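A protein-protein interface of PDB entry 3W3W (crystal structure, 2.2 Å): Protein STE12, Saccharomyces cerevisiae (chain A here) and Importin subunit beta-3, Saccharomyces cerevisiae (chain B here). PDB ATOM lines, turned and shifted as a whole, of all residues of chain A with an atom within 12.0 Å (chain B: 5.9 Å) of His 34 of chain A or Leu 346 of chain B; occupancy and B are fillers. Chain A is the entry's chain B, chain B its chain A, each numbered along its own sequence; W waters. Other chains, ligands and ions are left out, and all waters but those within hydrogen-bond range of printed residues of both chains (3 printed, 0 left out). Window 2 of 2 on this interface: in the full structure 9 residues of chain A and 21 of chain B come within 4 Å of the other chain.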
ATOM      1  N   SER A  30      19.053  15.804  11.721  1.00  0.00           N
ATOM      2  CA  SER A  30      18.085  15.638  10.625  1.00  0.00           C
ATOM      3  C   SER A  30      18.788  15.651   9.290  1.00  0.00           C
ATOM      4  O   SER A  30      19.931  16.058   9.182  1.00  0.00           O
ATOM      5  CB  SER A  30      17.050  16.777  10.634  1.00  0.00           C
ATOM      6  OG  SER A  30      17.693  18.048  10.515  1.00  0.00           O
ATOM      7  N   LYS A  31      18.101  15.206   8.247  1.00  0.00           N
ATOM      8  CA  LYS A  31      18.721  15.117   6.946  1.00  0.00           C
ATOM      9  C   LYS A  31      18.590  16.412   6.133  1.00  0.00           C
ATOM     10  O   LYS A  31      17.694  17.194   6.346  1.00  0.00           O
ATOM     11  CB  LYS A  31      18.105  14.001   6.189  1.00  0.00           C
ATOM     12  CG  LYS A  31      18.097  12.695   6.940  1.00  0.00           C
ATOM     13  CD  LYS A  31      17.816  11.567   5.992  1.00  0.00           C
ATOM     14  CE  LYS A  31      16.764  10.762   6.679  1.00  0.00           C
ATOM     15  NZ  LYS A  31      15.655  10.379   5.837  1.00  0.00           N
ATOM     16  N   PRO A  32      19.513  16.629   5.192  1.00  0.00           N
ATOM     17  CA  PRO A  32      19.455  17.815   4.333  1.00  0.00           C
ATOM     18  C   PRO A  32      18.209  17.765   3.476  1.00  0.00           C
ATOM     19  O   PRO A  32      17.706  16.665   3.186  1.00  0.00           O
ATOM     20  CB  PRO A  32      20.680  17.702   3.430  1.00  0.00           C
ATOM     21  CG  PRO A  32      21.522  16.609   4.021  1.00  0.00           C
ATOM     22  CD  PRO A  32      20.665  15.760   4.909  1.00  0.00           C
ATOM     23  N   LEU A  33      17.748  18.942   3.084  1.00  0.00           N
ATOM     24  CA  LEU A  33      16.529  19.107   2.289  1.00  0.00           C
ATOM     25  C   LEU A  33      16.689  18.544   0.910  1.00  0.00           C
ATOM     26  O   LEU A  33      17.755  18.619   0.340  1.00  0.00           O
ATOM     27  CB  LEU A  33      16.172  20.592   2.213  1.00  0.00           C
ATOM     28  CG  LEU A  33      14.767  20.791   2.818  1.00  0.00           C
ATOM     29  CD1 LEU A  33      13.788  19.848   2.101  1.00  0.00           C
ATOM     30  CD2 LEU A  33      14.713  20.576   4.335  1.00  0.00           C
ATOM     31  N   HIS A  34      15.636  17.974   0.342  1.00  0.00           N
ATOM     32  CA  HIS A  34      15.806  17.394  -1.008  1.00  0.00           C
ATOM     33  C   HIS A  34      16.101  18.434  -2.083  1.00  0.00           C
ATOM     34  O   HIS A  34      15.640  19.573  -1.981  1.00  0.00           O
ATOM     35  CB  HIS A  34      14.673  16.481  -1.402  1.00  0.00           C
ATOM     36  CG  HIS A  34      14.581  15.278  -0.523  1.00  0.00           C
ATOM     37  ND1 HIS A  34      13.546  14.371  -0.594  1.00  0.00           N
ATOM     38  CD2 HIS A  34      15.377  14.866   0.500  1.00  0.00           C
ATOM     39  CE1 HIS A  34      13.731  13.430   0.317  1.00  0.00           C
ATOM     40  NE2 HIS A  34      14.837  13.707   0.992  1.00  0.00           N
ATOM     41  N   ILE A  35      16.912  18.056  -3.074  1.00  0.00           N
ATOM     42  CA  ILE A  35      17.298  19.003  -4.130  1.00  0.00           C
ATOM     43  C   ILE A  35      16.748  18.696  -5.527  1.00  0.00           C
ATOM     44  O   ILE A  35      17.506  18.551  -6.441  1.00  0.00           O
ATOM     45  CB  ILE A  35      18.826  19.155  -4.281  1.00  0.00           C
ATOM     46  CG1 ILE A  35      19.509  19.400  -2.917  1.00  0.00           C
ATOM     47  CG2 ILE A  35      19.113  20.285  -5.275  1.00  0.00           C
ATOM     48  CD1 ILE A  35      20.940  19.907  -3.031  1.00  0.00           C
ATOM     49  N   LYS A  36      15.433  18.616  -5.700  1.00  0.00           N
ATOM     50  CA  LYS A  36      14.836  18.243  -7.031  1.00  0.00           C
ATOM     51  C   LYS A  36      14.315  19.486  -7.879  1.00  0.00           C
ATOM     52  O   LYS A  36      14.943  20.565  -7.784  1.00  0.00           O
ATOM     53  CB  LYS A  36      13.790  17.132  -6.821  1.00  0.00           C
ATOM     54  N   THR A  37      13.329  19.297  -8.791  1.00  0.00           N
ATOM     55  CA  THR A  37      12.088  20.158  -8.883  1.00  0.00           C
ATOM     56  C   THR A  37      10.879  19.448  -9.489  1.00  0.00           C
ATOM     57  O   THR A  37       9.754  19.660  -9.015  1.00  0.00           O
ATOM     58  CB  THR A  37      12.230  21.511  -9.599  1.00  0.00           C
ATOM     59  OG1 THR A  37      12.558  21.264 -10.961  1.00  0.00           O
ATOM     60  CG2 THR A  37      13.286  22.366  -8.952  1.00  0.00           C
ATOM     61  N   GLU B 283      12.526   7.432  -8.463  1.00  0.00           N
ATOM     62  CA  GLU B 283      11.252   8.116  -8.233  1.00  0.00           C
ATOM     63  C   GLU B 283      10.218   7.865  -9.320  1.00  0.00           C
ATOM     64  O   GLU B 283       9.068   8.131  -9.111  1.00  0.00           O
ATOM     65  CB  GLU B 283      11.469   9.644  -8.049  1.00  0.00           C
ATOM     66  CG  GLU B 283      11.860  10.017  -6.610  1.00  0.00           C
ATOM     67  CD  GLU B 283      12.894  11.149  -6.486  1.00  0.00           C
ATOM     68  OE1 GLU B 283      13.319  11.448  -5.346  1.00  0.00           O
ATOM     69  OE2 GLU B 283      13.284  11.764  -7.512  1.00  0.00           O
ATOM     70  N   GLN B 339      21.440  13.620   0.174  1.00  0.00           N
ATOM     71  CA  GLN B 339      20.006  13.702  -0.198  1.00  0.00           C
ATOM     72  C   GLN B 339      19.622  12.709  -1.267  1.00  0.00           C
ATOM     73  O   GLN B 339      18.515  12.225  -1.228  1.00  0.00           O
ATOM     74  CB  GLN B 339      19.563  15.150  -0.527  1.00  0.00           C
ATOM     75  CG  GLN B 339      20.205  15.795  -1.746  1.00  0.00           C
ATOM     76  CD  GLN B 339      19.541  15.463  -3.090  1.00  0.00           C
ATOM     77  OE1 GLN B 339      18.301  15.434  -3.217  1.00  0.00           O
ATOM     78  NE2 GLN B 339      20.375  15.218  -4.125  1.00  0.00           N
ATOM     79  N   LEU B 341      21.016   9.506  -1.668  1.00  0.00           N
ATOM     80  CA  LEU B 341      20.874   8.184  -1.026  1.00  0.00           C
ATOM     81  C   LEU B 341      19.557   8.135  -0.314  1.00  0.00           C
ATOM     82  O   LEU B 341      18.794   7.177  -0.399  1.00  0.00           O
ATOM     83  CB  LEU B 341      21.990   7.944   0.046  1.00  0.00           C
ATOM     84  CG  LEU B 341      22.548   6.503   0.128  1.00  0.00           C
ATOM     85  CD1 LEU B 341      23.371   6.229   1.397  1.00  0.00           C
ATOM     86  CD2 LEU B 341      21.472   5.430  -0.154  1.00  0.00           C
ATOM     87  N   ASP B 342      19.296   9.184   0.453  1.00  0.00           N
ATOM     88  CA  ASP B 342      18.067   9.284   1.229  1.00  0.00           C
ATOM     89  C   ASP B 342      16.941   9.117   0.254  1.00  0.00           C
ATOM     90  O   ASP B 342      16.089   8.235   0.419  1.00  0.00           O
ATOM     91  CB  ASP B 342      17.982  10.669   1.923  1.00  0.00           C
ATOM     92  CG  ASP B 342      16.660  10.867   2.716  1.00  0.00           C
ATOM     93  OD1 ASP B 342      16.118   9.878   3.239  1.00  0.00           O
ATOM     94  OD2 ASP B 342      16.176  12.005   2.884  1.00  0.00           O
ATOM     95  N   ARG B 343      16.913   9.929  -0.811  1.00  0.00           N
ATOM     96  CA  ARG B 343      15.767   9.819  -1.748  1.00  0.00           C
ATOM     97  C   ARG B 343      15.549   8.439  -2.356  1.00  0.00           C
ATOM     98  O   ARG B 343      14.426   7.945  -2.402  1.00  0.00           O
ATOM     99  CB  ARG B 343      15.899  10.820  -2.836  1.00  0.00           C
ATOM    100  CG  ARG B 343      15.438  12.220  -2.397  1.00  0.00           C
ATOM    101  CD  ARG B 343      16.104  13.212  -3.326  1.00  0.00           C
ATOM    102  NE  ARG B 343      15.518  13.093  -4.654  1.00  0.00           N
ATOM    103  CZ  ARG B 343      15.916  13.794  -5.708  1.00  0.00           C
ATOM    104  NH1 ARG B 343      16.985  14.569  -5.643  1.00  0.00           N
ATOM    105  NH2 ARG B 343      15.286  13.684  -6.863  1.00  0.00           N
ATOM    106  N   VAL B 344      16.597   7.793  -2.816  1.00  0.00           N
ATOM    107  CA  VAL B 344      16.436   6.462  -3.365  1.00  0.00           C
ATOM    108  C   VAL B 344      16.070   5.438  -2.285  1.00  0.00           C
ATOM    109  O   VAL B 344      15.180   4.613  -2.522  1.00  0.00           O
ATOM    110  CB  VAL B 344      17.681   6.030  -4.090  1.00  0.00           C
ATOM    111  CG1 VAL B 344      17.621   4.562  -4.499  1.00  0.00           C
ATOM    112  CG2 VAL B 344      17.870   6.905  -5.323  1.00  0.00           C
ATOM    113  N   ALA B 345      16.672   5.511  -1.078  1.00  0.00           N
ATOM    114  CA  ALA B 345      16.303   4.576  -0.038  1.00  0.00           C
ATOM    115  C   ALA B 345      14.801   4.692   0.216  1.00  0.00           C
ATOM    116  O   ALA B 345      14.144   3.703   0.421  1.00  0.00           O
ATOM    117  CB  ALA B 345      17.106   4.813   1.265  1.00  0.00           C
ATOM    118  N   LEU B 346      14.275   5.905   0.263  1.00  0.00           N
ATOM    119  CA  LEU B 346      12.915   6.111   0.608  1.00  0.00           C
ATOM    120  C   LEU B 346      11.986   5.513  -0.446  1.00  0.00           C
ATOM    121  O   LEU B 346      10.921   5.047  -0.124  1.00  0.00           O
ATOM    122  CB  LEU B 346      12.667   7.606   0.728  1.00  0.00           C
ATOM    123  CG  LEU B 346      13.132   8.401   1.968  1.00  0.00           C
ATOM    124  CD1 LEU B 346      12.879   9.884   1.696  1.00  0.00           C
ATOM    125  CD2 LEU B 346      12.442   7.940   3.269  1.00  0.00           C
ATOM    126  N   LYS B 347      12.391   5.562  -1.700  1.00  0.00           N
ATOM    127  CA  LYS B 347      11.636   4.981  -2.789  1.00  0.00           C
ATOM    128  C   LYS B 347      11.768   3.496  -2.929  1.00  0.00           C
ATOM    129  O   LYS B 347      10.794   2.842  -3.196  1.00  0.00           O
ATOM    130  CB  LYS B 347      12.053   5.622  -4.127  1.00  0.00           C
ATOM    131  CG  LYS B 347      11.596   7.057  -4.207  1.00  0.00           C
ATOM    132  CD  LYS B 347      10.080   7.153  -3.941  1.00  0.00           C
ATOM    133  CE  LYS B 347       9.625   8.571  -4.229  1.00  0.00           C
ATOM    134  NZ  LYS B 347       8.171   8.642  -3.898  1.00  0.00           N
ATOM    135  N   LEU B 348      12.968   2.954  -2.766  1.00  0.00           N
ATOM    136  CA  LEU B 348      13.206   1.531  -3.050  1.00  0.00           C
ATOM    137  C   LEU B 348      13.141   0.540  -1.844  1.00  0.00           C
ATOM    138  O   LEU B 348      12.839  -0.649  -2.044  1.00  0.00           O
ATOM    139  CB  LEU B 348      14.488   1.331  -3.873  1.00  0.00           C
ATOM    140  CG  LEU B 348      14.630   2.165  -5.162  1.00  0.00           C
ATOM    141  CD1 LEU B 348      15.898   1.794  -5.900  1.00  0.00           C
ATOM    142  CD2 LEU B 348      13.430   2.034  -6.087  1.00  0.00           C
ATOM    143  N   GLY B 349      13.422   1.006  -0.619  1.00  0.00           N
ATOM    144  CA  GLY B 349      13.202   0.147   0.545  1.00  0.00           C
ATOM    145  C   GLY B 349      14.455  -0.671   0.834  1.00  0.00           C
ATOM    146  O   GLY B 349      15.411  -0.686   0.031  1.00  0.00           O
ATOM    147  N   GLU B 385      16.152   5.684   7.187  1.00  0.00           N
ATOM    148  CA  GLU B 385      14.702   5.752   7.163  1.00  0.00           C
ATOM    149  C   GLU B 385      14.108   4.907   6.061  1.00  0.00           C
ATOM    150  O   GLU B 385      13.181   4.108   6.273  1.00  0.00           O
ATOM    151  CB  GLU B 385      14.226   7.205   6.991  1.00  0.00           C
ATOM    152  CG  GLU B 385      12.714   7.321   6.879  1.00  0.00           C
ATOM    153  CD  GLU B 385      12.234   8.760   6.671  1.00  0.00           C
ATOM    154  OE1 GLU B 385      13.066   9.707   6.612  1.00  0.00           O
ATOM    155  OE2 GLU B 385      10.993   8.950   6.526  1.00  0.00           O
ATOM    156  N   GLY B 386      14.620   5.090   4.856  1.00  0.00           N
ATOM    157  CA  GLY B 386      14.049   4.333   3.743  1.00  0.00           C
ATOM    158  C   GLY B 386      14.251   2.838   3.858  1.00  0.00           C
ATOM    159  O   GLY B 386      13.425   2.070   3.399  1.00  0.00           O
ATOM    160  N   CYS B 387      15.343   2.438   4.493  1.00  0.00           N
ATOM    161  CA  CYS B 387      15.637   1.027   4.717  1.00  0.00           C
ATOM    162  C   CYS B 387      15.154   0.499   6.086  1.00  0.00           C
ATOM    163  O   CYS B 387      15.496  -0.592   6.449  1.00  0.00           O
ATOM    164  CB  CYS B 387      17.126   0.828   4.630  1.00  0.00           C
ATOM    165  SG  CYS B 387      17.859   1.157   3.021  1.00  0.00           S
HETATM  166  O   HOH W   1      17.341   8.153   7.505  1.00  0.00           O
HETATM  167  O   HOH W   2      14.078  13.008   4.047  1.00  0.00           O
HETATM  168  O   HOH W   3      18.284  13.837   2.784  1.00  0.00           O
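Water W2 bridges OD2 of Asp 342 of chain B (2.6 Å) and NE2 of His 34 of chain A (3.2 Å). Water W1 bridges N of Glu 385 of chain B (2.8 Å) and NZ of Lys 31 of chain A (3.3 Å). Water W3 bridges OD2 of Asp 342 of chain B (2.8 Å) and O of Pro 32 of chain A (2.9 Å).
Among the printed residues, merely in contact across the chains: His 34 of chain A with Arg 343 of chain B (3.4 Å), Lys 36 of chain A with Arg 343 of chain B (3.8 Å), His 34 of chain A with Gln 339 of chain B (3.9 Å) and His 34 of chain A with Leu 346 of chain B (3.9 Å).
His 34 of chain A touches four residues of chain B. Asp 342 of chain B touches two residues of chain A. Of chain A, only His 34 and Lys 36 come within 4 Å of Arg 343 of chain B. No residue of chain A comes within 4 Å of Val 344 of chain B. No residue of chain A comes within 4 Å of Lys 347 of chain B. No residue of chain A comes within 4 Å of Leu 348 of chain B. No residue of chain A comes within 4 Å of Gly 349 of chain B. Of the printed residues of chain B, Lys 31 of chain A touches Asp 342 and Glu 385. Printed residues of chain B within 4 Å of Lys 36 of chain A: Arg 343. Pro 32 of chain A touches none of the printed residues of chain B. Glu 283 of chain B touches none of the printed residues of chain A.
The side-chain amide oxygen (OE1) of Gln 339 of chain B lies within hydrogen-bond range of the backbone NH (N) of Ile 35 of chain A (3.0 Å). The side-chain amino group (NZ) of Lys 31 of chain A is in salt-bridge range of the side-chain carboxylate (OD1) of Asp 342 of chain B (2.7 Å). The side-chain carboxylate of Asp 342 of chain B sits at hydrogen-bond distance from a ring nitrogen (NE2) of His 34 of chain A (2.9 Å). The side-chain amino group of Lys 31 of chain A is in salt-bridge range of the side-chain carboxylate of Glu 385 of chain B.
Hydrophobic or aromatic side chains of chain A within 4 Å of the printed part of chain B: His 34 and Ile 35. Of the 14 printed residues of chain B, 5 touch a printed residue of chain A. Among the printed residues, 8 pairs touch across the chains.
The side-chain carboxylate (OE1) of Glu 283 of chain B is in salt-bridge range of the guanidinium group (NE) of Arg 343 of chain B (2.8 Å). The side-chain amide oxygen (OE1) of Gln 339 of chain B lies within hydrogen-bond range of the guanidinium group (NH1) of Arg 343 of chain B (2.9 Å).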
